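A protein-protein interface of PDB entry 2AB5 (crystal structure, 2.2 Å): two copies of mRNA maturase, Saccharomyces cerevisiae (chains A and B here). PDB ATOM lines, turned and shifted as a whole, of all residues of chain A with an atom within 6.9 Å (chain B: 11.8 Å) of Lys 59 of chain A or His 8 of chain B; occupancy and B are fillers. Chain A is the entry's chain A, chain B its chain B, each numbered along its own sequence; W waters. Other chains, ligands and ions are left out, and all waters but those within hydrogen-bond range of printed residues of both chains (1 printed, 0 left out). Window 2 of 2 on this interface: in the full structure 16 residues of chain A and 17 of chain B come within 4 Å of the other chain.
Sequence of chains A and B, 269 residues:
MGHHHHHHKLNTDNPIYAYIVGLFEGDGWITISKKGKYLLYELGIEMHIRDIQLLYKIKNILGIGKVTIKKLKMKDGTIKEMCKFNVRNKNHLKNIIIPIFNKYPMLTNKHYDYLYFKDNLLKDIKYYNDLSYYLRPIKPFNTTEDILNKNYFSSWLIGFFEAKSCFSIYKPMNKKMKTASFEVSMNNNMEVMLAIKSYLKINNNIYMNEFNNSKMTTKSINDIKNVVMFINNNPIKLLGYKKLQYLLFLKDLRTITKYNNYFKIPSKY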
ATOM      1  N   LEU A  54     -10.184  -7.134  -4.786  1.00  0.00           N
ATOM      2  CA  LEU A  54      -9.422  -6.162  -4.016  1.00  0.00           C
ATOM      3  C   LEU A  54      -8.260  -6.863  -3.292  1.00  0.00           C
ATOM      4  O   LEU A  54      -7.152  -6.322  -3.214  1.00  0.00           O
ATOM      5  CB  LEU A  54     -10.327  -5.474  -2.988  1.00  0.00           C
ATOM      6  CG  LEU A  54      -9.617  -4.602  -1.956  1.00  0.00           C
ATOM      7  CD1 LEU A  54      -8.739  -3.581  -2.662  1.00  0.00           C
ATOM      8  CD2 LEU A  54     -10.643  -3.918  -1.090  1.00  0.00           C
ATOM      9  N   LEU A  55      -8.509  -8.054  -2.747  1.00  0.00           N
ATOM     10  CA  LEU A  55      -7.437  -8.767  -2.054  1.00  0.00           C
ATOM     11  C   LEU A  55      -6.323  -9.096  -3.050  1.00  0.00           C
ATOM     12  O   LEU A  55      -5.140  -8.973  -2.729  1.00  0.00           O
ATOM     13  CB  LEU A  55      -7.971 -10.028  -1.362  1.00  0.00           C
ATOM     14  CG  LEU A  55      -9.017  -9.781  -0.271  1.00  0.00           C
ATOM     15  CD1 LEU A  55      -9.198 -11.052   0.553  1.00  0.00           C
ATOM     16  CD2 LEU A  55      -8.579  -8.630   0.652  1.00  0.00           C
ATOM     17  N   TYR A  56      -6.697  -9.468  -4.273  1.00  0.00           N
ATOM     18  CA  TYR A  56      -5.705  -9.754  -5.305  1.00  0.00           C
ATOM     19  C   TYR A  56      -4.899  -8.509  -5.692  1.00  0.00           C
ATOM     20  O   TYR A  56      -3.734  -8.620  -6.093  1.00  0.00           O
ATOM     21  CB  TYR A  56      -6.359 -10.357  -6.551  1.00  0.00           C
ATOM     22  CG  TYR A  56      -6.484 -11.854  -6.447  1.00  0.00           C
ATOM     23  CD1 TYR A  56      -7.703 -12.451  -6.121  1.00  0.00           C
ATOM     24  CD2 TYR A  56      -5.360 -12.671  -6.570  1.00  0.00           C
ATOM     25  CE1 TYR A  56      -7.800 -13.828  -5.905  1.00  0.00           C
ATOM     26  CE2 TYR A  56      -5.444 -14.051  -6.349  1.00  0.00           C
ATOM     27  CZ  TYR A  56      -6.665 -14.614  -6.013  1.00  0.00           C
ATOM     28  OH  TYR A  56      -6.745 -15.947  -5.720  1.00  0.00           O
ATOM     29  N   LYS A  57      -5.520  -7.332  -5.598  1.00  0.00           N
ATOM     30  CA  LYS A  57      -4.808  -6.090  -5.890  1.00  0.00           C
ATOM     31  C   LYS A  57      -3.779  -5.877  -4.772  1.00  0.00           C
ATOM     32  O   LYS A  57      -2.621  -5.578  -5.039  1.00  0.00           O
ATOM     33  CB  LYS A  57      -5.783  -4.905  -5.953  1.00  0.00           C
ATOM     34  CG  LYS A  57      -6.578  -4.847  -7.254  1.00  0.00           C
ATOM     35  CD  LYS A  57      -7.574  -3.709  -7.244  1.00  0.00           C
ATOM     36  CE  LYS A  57      -8.337  -3.657  -8.563  1.00  0.00           C
ATOM     37  NZ  LYS A  57      -9.383  -2.592  -8.518  1.00  0.00           N
ATOM     38  N   ILE A  58      -4.207  -6.033  -3.522  1.00  0.00           N
ATOM     39  CA  ILE A  58      -3.296  -5.898  -2.388  1.00  0.00           C
ATOM     40  C   ILE A  58      -2.084  -6.824  -2.612  1.00  0.00           C
ATOM     41  O   ILE A  58      -0.942  -6.389  -2.546  1.00  0.00           O
ATOM     42  CB  ILE A  58      -4.003  -6.287  -1.059  1.00  0.00           C
ATOM     43  CG1 ILE A  58      -5.236  -5.404  -0.852  1.00  0.00           C
ATOM     44  CG2 ILE A  58      -3.025  -6.187   0.130  1.00  0.00           C
ATOM     45  CD1 ILE A  58      -5.026  -3.952  -1.186  1.00  0.00           C
ATOM     46  N   LYS A  59      -2.357  -8.095  -2.906  1.00  0.00           N
ATOM     47  CA  LYS A  59      -1.321  -9.101  -3.149  1.00  0.00           C
ATOM     48  C   LYS A  59      -0.301  -8.673  -4.207  1.00  0.00           C
ATOM     49  O   LYS A  59       0.913  -8.815  -4.016  1.00  0.00           O
ATOM     50  CB  LYS A  59      -1.963 -10.425  -3.589  1.00  0.00           C
ATOM     51  CG  LYS A  59      -0.963 -11.511  -3.965  1.00  0.00           C
ATOM     52  CD  LYS A  59      -1.655 -12.757  -4.524  1.00  0.00           C
ATOM     53  CE  LYS A  59      -0.627 -13.801  -4.944  1.00  0.00           C
ATOM     54  NZ  LYS A  59      -1.221 -14.886  -5.769  1.00  0.00           N
ATOM     55  N   ASN A  60      -0.797  -8.160  -5.326  1.00  0.00           N
ATOM     56  CA  ASN A  60       0.074  -7.726  -6.401  1.00  0.00           C
ATOM     57  C   ASN A  60       0.826  -6.446  -6.095  1.00  0.00           C
ATOM     58  O   ASN A  60       1.925  -6.236  -6.588  1.00  0.00           O
ATOM     59  CB  ASN A  60      -0.740  -7.576  -7.672  1.00  0.00           C
ATOM     60  CG  ASN A  60      -1.084  -8.913  -8.283  1.00  0.00           C
ATOM     61  OD1 ASN A  60      -0.251  -9.522  -8.953  1.00  0.00           O
ATOM     62  ND2 ASN A  60      -2.299  -9.392  -8.036  1.00  0.00           N
ATOM     63  N   ILE A  61       0.230  -5.588  -5.279  1.00  0.00           N
ATOM     64  CA  ILE A  61       0.868  -4.337  -4.892  1.00  0.00           C
ATOM     65  C   ILE A  61       1.975  -4.583  -3.852  1.00  0.00           C
ATOM     66  O   ILE A  61       3.032  -3.952  -3.892  1.00  0.00           O
ATOM     67  CB  ILE A  61      -0.150  -3.376  -4.272  1.00  0.00           C
ATOM     68  CG1 ILE A  61      -1.145  -2.913  -5.337  1.00  0.00           C
ATOM     69  CG2 ILE A  61       0.579  -2.214  -3.607  1.00  0.00           C
ATOM     70  CD1 ILE A  61      -2.307  -2.116  -4.758  1.00  0.00           C
ATOM     71  N   LEU A  62       1.722  -5.477  -2.905  1.00  0.00           N
ATOM     72  CA  LEU A  62       2.714  -5.769  -1.884  1.00  0.00           C
ATOM     73  C   LEU A  62       3.770  -6.741  -2.414  1.00  0.00           C
ATOM     74  O   LEU A  62       4.887  -6.770  -1.905  1.00  0.00           O
ATOM     75  CB  LEU A  62       2.043  -6.338  -0.637  1.00  0.00           C
ATOM     76  CG  LEU A  62       1.178  -5.375   0.159  1.00  0.00           C
ATOM     77  CD1 LEU A  62       0.493  -6.098   1.303  1.00  0.00           C
ATOM     78  CD2 LEU A  62       2.043  -4.240   0.690  1.00  0.00           C
ATOM     79  N   GLY A  63       3.402  -7.522  -3.431  1.00  0.00           N
ATOM     80  CA  GLY A  63       4.315  -8.479  -4.041  1.00  0.00           C
ATOM     81  C   GLY A  63       4.545  -9.748  -3.232  1.00  0.00           C
ATOM     82  O   GLY A  63       5.427 -10.547  -3.541  1.00  0.00           O
ATOM     83  N   ILE A  64       3.742  -9.936  -2.193  1.00  0.00           N
ATOM     84  CA  ILE A  64       3.849 -11.093  -1.313  1.00  0.00           C
ATOM     85  C   ILE A  64       2.456 -11.479  -0.834  1.00  0.00           C
ATOM     86  O   ILE A  64       1.479 -10.796  -1.139  1.00  0.00           O
ATOM     87  CB  ILE A  64       4.686 -10.748  -0.077  1.00  0.00           C
ATOM     88  CG1 ILE A  64       4.136  -9.466   0.562  1.00  0.00           C
ATOM     89  CG2 ILE A  64       6.142 -10.593  -0.470  1.00  0.00           C
ATOM     90  CD1 ILE A  64       4.691  -9.163   1.928  1.00  0.00           C
ATOM     91  N   GLY A  65       2.373 -12.574  -0.082  1.00  0.00           N
ATOM     92  CA  GLY A  65       1.098 -12.997   0.470  1.00  0.00           C
ATOM     93  C   GLY A  65       0.285 -13.987  -0.330  1.00  0.00           C
ATOM     94  O   GLY A  65       0.623 -14.320  -1.451  1.00  0.00           O
ATOM     95  N   LYS A  66      -0.814 -14.438   0.263  1.00  0.00           N
ATOM     96  CA  LYS A  66      -1.694 -15.401  -0.371  1.00  0.00           C
ATOM     97  C   LYS A  66      -3.165 -15.088  -0.170  1.00  0.00           C
ATOM     98  O   LYS A  66      -3.571 -14.626   0.886  1.00  0.00           O
ATOM     99  CB  LYS A  66      -1.373 -16.801   0.161  1.00  0.00           C
ATOM    100  CG  LYS A  66      -0.059 -17.318  -0.403  1.00  0.00           C
ATOM    101  CD  LYS A  66       0.561 -18.418   0.417  1.00  0.00           C
ATOM    102  CE  LYS A  66       1.905 -18.796  -0.187  1.00  0.00           C
ATOM    103  NZ  LYS A  66       2.747 -17.590  -0.486  1.00  0.00           N
ATOM    104  N   VAL A  67      -3.955 -15.337  -1.205  1.00  0.00           N
ATOM    105  CA  VAL A  67      -5.392 -15.110  -1.143  1.00  0.00           C
ATOM    106  C   VAL A  67      -6.084 -16.460  -1.088  1.00  0.00           C
ATOM    107  O   VAL A  67      -5.753 -17.358  -1.841  1.00  0.00           O
ATOM    108  CB  VAL A  67      -5.911 -14.369  -2.384  1.00  0.00           C
ATOM    109  CG1 VAL A  67      -7.428 -14.315  -2.333  1.00  0.00           C
ATOM    110  CG2 VAL A  67      -5.308 -12.966  -2.449  1.00  0.00           C
ATOM    111  N   PHE A  85      -6.647 -12.590   2.891  1.00  0.00           N
ATOM    112  CA  PHE A  85      -5.308 -12.331   2.407  1.00  0.00           C
ATOM    113  C   PHE A  85      -4.433 -12.301   3.654  1.00  0.00           C
ATOM    114  O   PHE A  85      -4.809 -11.701   4.665  1.00  0.00           O
ATOM    115  CB  PHE A  85      -5.233 -10.978   1.701  1.00  0.00           C
ATOM    116  CG  PHE A  85      -3.829 -10.537   1.411  1.00  0.00           C
ATOM    117  CD1 PHE A  85      -3.138 -11.047   0.321  1.00  0.00           C
ATOM    118  CD2 PHE A  85      -3.161  -9.686   2.296  1.00  0.00           C
ATOM    119  CE1 PHE A  85      -1.802 -10.727   0.116  1.00  0.00           C
ATOM    120  CE2 PHE A  85      -1.834  -9.360   2.102  1.00  0.00           C
ATOM    121  CZ  PHE A  85      -1.147  -9.883   1.009  1.00  0.00           C
ATOM    122  N   HIS B   8       1.468 -13.420 -12.200  1.00  0.00           N
ATOM    123  CA  HIS B   8       0.294 -12.534 -12.439  1.00  0.00           C
ATOM    124  C   HIS B   8       0.736 -11.315 -13.250  1.00  0.00           C
ATOM    125  O   HIS B   8       1.879 -11.246 -13.699  1.00  0.00           O
ATOM    126  CB  HIS B   8      -0.308 -12.081 -11.103  1.00  0.00           C
ATOM    127  CG  HIS B   8      -0.697 -13.212 -10.198  1.00  0.00           C
ATOM    128  ND1 HIS B   8       0.216 -14.119  -9.701  1.00  0.00           N
ATOM    129  CD2 HIS B   8      -1.902 -13.583  -9.700  1.00  0.00           C
ATOM    130  CE1 HIS B   8      -0.408 -14.999  -8.939  1.00  0.00           C
ATOM    131  NE2 HIS B   8      -1.693 -14.696  -8.922  1.00  0.00           N
ATOM    132  N   LYS B   9      -0.172 -10.359 -13.433  1.00  0.00           N
ATOM    133  CA  LYS B   9       0.130  -9.143 -14.189  1.00  0.00           C
ATOM    134  C   LYS B   9       0.324  -7.927 -13.277  1.00  0.00           C
ATOM    135  O   LYS B   9      -0.049  -7.959 -12.102  1.00  0.00           O
ATOM    136  CB  LYS B   9      -0.975  -8.866 -15.219  1.00  0.00           C
ATOM    137  CG  LYS B   9      -1.095  -9.955 -16.272  1.00  0.00           C
ATOM    138  CD  LYS B   9      -1.830  -9.470 -17.510  1.00  0.00           C
ATOM    139  CE  LYS B   9      -1.677 -10.470 -18.648  1.00  0.00           C
ATOM    140  NZ  LYS B   9      -2.104  -9.901 -19.958  1.00  0.00           N
ATOM    141  N   LEU B  10       0.905  -6.860 -13.829  1.00  0.00           N
ATOM    142  CA  LEU B  10       1.195  -5.638 -13.075  1.00  0.00           C
ATOM    143  C   LEU B  10      -0.014  -4.782 -12.693  1.00  0.00           C
ATOM    144  O   LEU B  10      -0.729  -4.275 -13.558  1.00  0.00           O
ATOM    145  CB  LEU B  10       2.201  -4.770 -13.853  1.00  0.00           C
ATOM    146  CG  LEU B  10       2.740  -3.508 -13.164  1.00  0.00           C
ATOM    147  CD1 LEU B  10       3.615  -3.897 -11.977  1.00  0.00           C
ATOM    148  CD2 LEU B  10       3.540  -2.674 -14.159  1.00  0.00           C
ATOM    149  N   ASN B  11      -0.235  -4.624 -11.391  1.00  0.00           N
ATOM    150  CA  ASN B  11      -1.333  -3.795 -10.910  1.00  0.00           C
ATOM    151  C   ASN B  11      -0.899  -2.337 -11.121  1.00  0.00           C
ATOM    152  O   ASN B  11       0.168  -1.919 -10.650  1.00  0.00           O
ATOM    153  CB  ASN B  11      -1.587  -4.049  -9.427  1.00  0.00           C
ATOM    154  CG  ASN B  11      -2.840  -3.357  -8.932  1.00  0.00           C
ATOM    155  OD1 ASN B  11      -3.952  -3.848  -9.122  1.00  0.00           O
ATOM    156  ND2 ASN B  11      -2.667  -2.198  -8.311  1.00  0.00           N
ATOM    157  N   THR B  12      -1.732  -1.567 -11.814  1.00  0.00           N
ATOM    158  CA  THR B  12      -1.410  -0.184 -12.133  1.00  0.00           C
ATOM    159  C   THR B  12      -2.334   0.908 -11.571  1.00  0.00           C
ATOM    160  O   THR B  12      -2.304   2.039 -12.055  1.00  0.00           O
ATOM    161  CB  THR B  12      -1.340  -0.008 -13.675  1.00  0.00           C
ATOM    162  OG1 THR B  12      -2.542  -0.516 -14.266  1.00  0.00           O
ATOM    163  CG2 THR B  12      -0.144  -0.760 -14.259  1.00  0.00           C
ATOM    164  N   ASP B  13      -3.148   0.597 -10.564  1.00  0.00           N
ATOM    165  CA  ASP B  13      -4.036   1.617  -9.995  1.00  0.00           C
ATOM    166  C   ASP B  13      -3.303   2.579  -9.034  1.00  0.00           C
ATOM    167  O   ASP B  13      -3.934   3.403  -8.376  1.00  0.00           O
ATOM    168  CB  ASP B  13      -5.211   0.960  -9.263  1.00  0.00           C
ATOM    169  CG  ASP B  13      -5.352  -0.510  -9.591  1.00  0.00           C
ATOM    170  OD1 ASP B  13      -5.458  -0.843 -10.788  1.00  0.00           O
ATOM    171  OD2 ASP B  13      -5.351  -1.334  -8.651  1.00  0.00           O
ATOM    172  N   ASN B  14      -1.977   2.461  -8.961  1.00  0.00           N
ATOM    173  CA  ASN B  14      -1.163   3.321  -8.108  1.00  0.00           C
ATOM    174  C   ASN B  14      -0.675   4.570  -8.856  1.00  0.00           C
ATOM    175  O   ASN B  14       0.059   4.476  -9.846  1.00  0.00           O
ATOM    176  CB  ASN B  14       0.030   2.532  -7.549  1.00  0.00           C
ATOM    177  CG  ASN B  14       1.032   3.413  -6.817  1.00  0.00           C
ATOM    178  OD1 ASN B  14       0.701   4.481  -6.265  1.00  0.00           O
ATOM    179  ND2 ASN B  14       2.278   2.957  -6.800  1.00  0.00           N
ATOM    180  N   TYR B  17       2.793   5.833 -10.498  1.00  0.00           N
ATOM    181  CA  TYR B  17       3.184   5.402 -11.843  1.00  0.00           C
ATOM    182  C   TYR B  17       2.885   6.541 -12.823  1.00  0.00           C
ATOM    183  O   TYR B  17       3.509   6.661 -13.872  1.00  0.00           O
ATOM    184  CB  TYR B  17       2.414   4.138 -12.244  1.00  0.00           C
ATOM    185  CG  TYR B  17       2.930   2.860 -11.606  1.00  0.00           C
ATOM    186  CD1 TYR B  17       2.059   1.814 -11.281  1.00  0.00           C
ATOM    187  CD2 TYR B  17       4.291   2.688 -11.340  1.00  0.00           C
ATOM    188  CE1 TYR B  17       2.537   0.633 -10.702  1.00  0.00           C
ATOM    189  CE2 TYR B  17       4.774   1.513 -10.761  1.00  0.00           C
ATOM    190  CZ  TYR B  17       3.894   0.497 -10.446  1.00  0.00           C
ATOM    191  OH  TYR B  17       4.374  -0.651  -9.862  1.00  0.00           O
ATOM    192  N   ASN B  91      11.462  -8.283 -22.279  1.00  0.00           N
ATOM    193  CA  ASN B  91      10.388  -8.818 -21.457  1.00  0.00           C
ATOM    194  C   ASN B  91      10.025  -7.838 -20.347  1.00  0.00           C
ATOM    195  O   ASN B  91       8.863  -7.722 -19.980  1.00  0.00           O
ATOM    196  CB  ASN B  91      10.760 -10.190 -20.879  1.00  0.00           C
ATOM    197  CG  ASN B  91      10.655 -11.304 -21.914  1.00  0.00           C
ATOM    198  OD1 ASN B  91       9.729 -11.329 -22.727  1.00  0.00           O
ATOM    199  ND2 ASN B  91      11.601 -12.238 -21.880  1.00  0.00           N
ATOM    200  N   HIS B  92      11.015  -7.121 -19.819  1.00  0.00           N
ATOM    201  CA  HIS B  92      10.757  -6.140 -18.765  1.00  0.00           C
ATOM    202  C   HIS B  92       9.940  -4.985 -19.321  1.00  0.00           C
ATOM    203  O   HIS B  92       9.054  -4.468 -18.656  1.00  0.00           O
ATOM    204  CB  HIS B  92      12.073  -5.619 -18.197  1.00  0.00           C
ATOM    205  CG  HIS B  92      12.780  -6.613 -17.342  1.00  0.00           C
ATOM    206  ND1 HIS B  92      14.071  -6.433 -16.900  1.00  0.00           N
ATOM    207  CD2 HIS B  92      12.370  -7.802 -16.839  1.00  0.00           C
ATOM    208  CE1 HIS B  92      14.429  -7.470 -16.164  1.00  0.00           C
ATOM    209  NE2 HIS B  92      13.414  -8.316 -16.112  1.00  0.00           N
ATOM    210  N   LYS B  94       7.921  -5.134 -21.998  1.00  0.00           N
ATOM    211  CA  LYS B  94       6.575  -5.649 -22.294  1.00  0.00           C
ATOM    212  C   LYS B  94       5.726  -5.859 -21.049  1.00  0.00           C
ATOM    213  O   LYS B  94       4.520  -5.590 -21.051  1.00  0.00           O
ATOM    214  CB  LYS B  94       6.638  -6.984 -23.038  1.00  0.00           C
ATOM    215  CG  LYS B  94       7.268  -6.946 -24.417  1.00  0.00           C
ATOM    216  CD  LYS B  94       7.049  -8.285 -25.091  1.00  0.00           C
ATOM    217  CE  LYS B  94       7.678  -8.365 -26.460  1.00  0.00           C
ATOM    218  NZ  LYS B  94       7.361  -9.695 -27.103  1.00  0.00           N
ATOM    219  N   ASN B  95       6.350  -6.336 -19.980  1.00  0.00           N
ATOM    220  CA  ASN B  95       5.609  -6.602 -18.762  1.00  0.00           C
ATOM    221  C   ASN B  95       5.454  -5.476 -17.742  1.00  0.00           C
ATOM    222  O   ASN B  95       4.497  -5.487 -16.971  1.00  0.00           O
ATOM    223  CB  ASN B  95       6.205  -7.818 -18.061  1.00  0.00           C
ATOM    224  CG  ASN B  95       6.192  -9.052 -18.939  1.00  0.00           C
ATOM    225  OD1 ASN B  95       5.290  -9.226 -19.761  1.00  0.00           O
ATOM    226  ND2 ASN B  95       7.187  -9.922 -18.762  1.00  0.00           N
ATOM    227  N   ILE B  96       6.370  -4.515 -17.713  1.00  0.00           N
ATOM    228  CA  ILE B  96       6.246  -3.460 -16.721  1.00  0.00           C
ATOM    229  C   ILE B  96       5.907  -2.118 -17.337  1.00  0.00           C
ATOM    230  O   ILE B  96       4.901  -1.504 -16.990  1.00  0.00           O
ATOM    231  CB  ILE B  96       7.558  -3.287 -15.896  1.00  0.00           C
ATOM    232  CG1 ILE B  96       7.990  -4.627 -15.297  1.00  0.00           C
ATOM    233  CG2 ILE B  96       7.351  -2.249 -14.790  1.00  0.00           C
ATOM    234  CD1 ILE B  96       6.974  -5.244 -14.397  1.00  0.00           C
ATOM    235  N   ILE B  97       6.759  -1.689 -18.259  1.00  0.00           N
ATOM    236  CA  ILE B  97       6.633  -0.401 -18.924  1.00  0.00           C
ATOM    237  C   ILE B  97       5.389  -0.216 -19.795  1.00  0.00           C
ATOM    238  O   ILE B  97       4.717   0.827 -19.726  1.00  0.00           O
ATOM    239  CB  ILE B  97       7.890  -0.134 -19.759  1.00  0.00           C
ATOM    240  CG1 ILE B  97       9.135  -0.344 -18.878  1.00  0.00           C
ATOM    241  CG2 ILE B  97       7.842   1.271 -20.363  1.00  0.00           C
ATOM    242  CD1 ILE B  97       9.041   0.284 -17.499  1.00  0.00           C
ATOM    243  N   PRO B  99       2.393  -1.690 -19.631  1.00  0.00           N
ATOM    244  CA  PRO B  99       1.212  -1.525 -18.776  1.00  0.00           C
ATOM    245  C   PRO B  99       1.166  -0.173 -18.060  1.00  0.00           C
ATOM    246  O   PRO B  99       0.099   0.405 -17.894  1.00  0.00           O
ATOM    247  CB  PRO B  99       1.333  -2.686 -17.801  1.00  0.00           C
ATOM    248  CG  PRO B  99       2.035  -3.745 -18.635  1.00  0.00           C
ATOM    249  CD  PRO B  99       3.104  -2.942 -19.307  1.00  0.00           C
HETATM  250  O   HOH W   1       1.212  -6.561  -9.375  1.00  0.00           O
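NE2 of His 8 of chain B lies within hydrogen-bond range of NZ of Lys 59 of chain A (3.2 Å).
The side-chain amide nitrogen (ND2) of Asn 60 of chain A is in hydrogen-bond range of the backbone carbonyl oxygen (O) of Tyr 56 of chain A (2.5 Å). The side-chain amide nitrogen (ND2) of Asn 11 of chain B lies within hydrogen-bond range of the side-chain carboxylate (OD2) of Asp 13 of chain B, 2.8 Å away.
Among the printed residues, merely in contact across the chains: Asn 60 of chain A with His 8 of chain B, Lys 57 of chain A with Asn 11 of chain B, Ile 61 of chain A with Asn 11 of chain B, Asn 60 of chain A with Lys 9 of chain B and Lys 57 of chain A with Asp 13 of chain B.
Lys 59 of chain A touches just one residue of chain B: His 8. Tyr 56 of chain A touches none of the printed residues of chain B. No residue of chain B comes within 4 Å of Ile 58 of chain A. Ile 61 of chain A touches just one residue of chain B: Asn 11. No residue of chain B comes within 4 Å of Leu 62 of chain A. No residue of chain B comes within 4 Å of Gly 63 of chain A. No residue of chain B comes within 4 Å of Gly 65 of chain A. No residue of chain B comes within 4 Å of Lys 66 of chain A. No residue of chain B comes within 4 Å of Val 67 of chain A. Printed residues of chain A within 4 Å of Asp 13 of chain B: Lys 57 (3.5 Å). Of the printed residues of chain B, Lys 57 of chain A touches Asn 11 (3.4 Å) and Asp 13 (3.5 Å). Printed residues of chain A within 4 Å of Asn 11 of chain B: Lys 57 and Ile 61. Printed residues of chain A within 4 Å of Lys 9 of chain B: Asn 60. Phe 85 of chain A touches none of the printed residues of chain B.
Hydrophobic or aromatic side chains of chain A within 4 Å of the printed part of chain B: Ile 61. Among the printed residues, 6 pairs touch across the chains. Among the printed residues, no Asp or Glu carboxylate lies within 4 Å of a Lys or Arg side-chain nitrogen of the other chain.
No position is printed for both chains.
Water W1 lies within hydrogen-bond range of the backbone carbonyl oxygen (O) of Asn 60 of chain A (2.9 Å), the backbone NH (N) of Asn 11 of chain B (3.1 Å) and the backbone carbonyl oxygen (O) of Lys 9 of chain B (3.3 Å).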
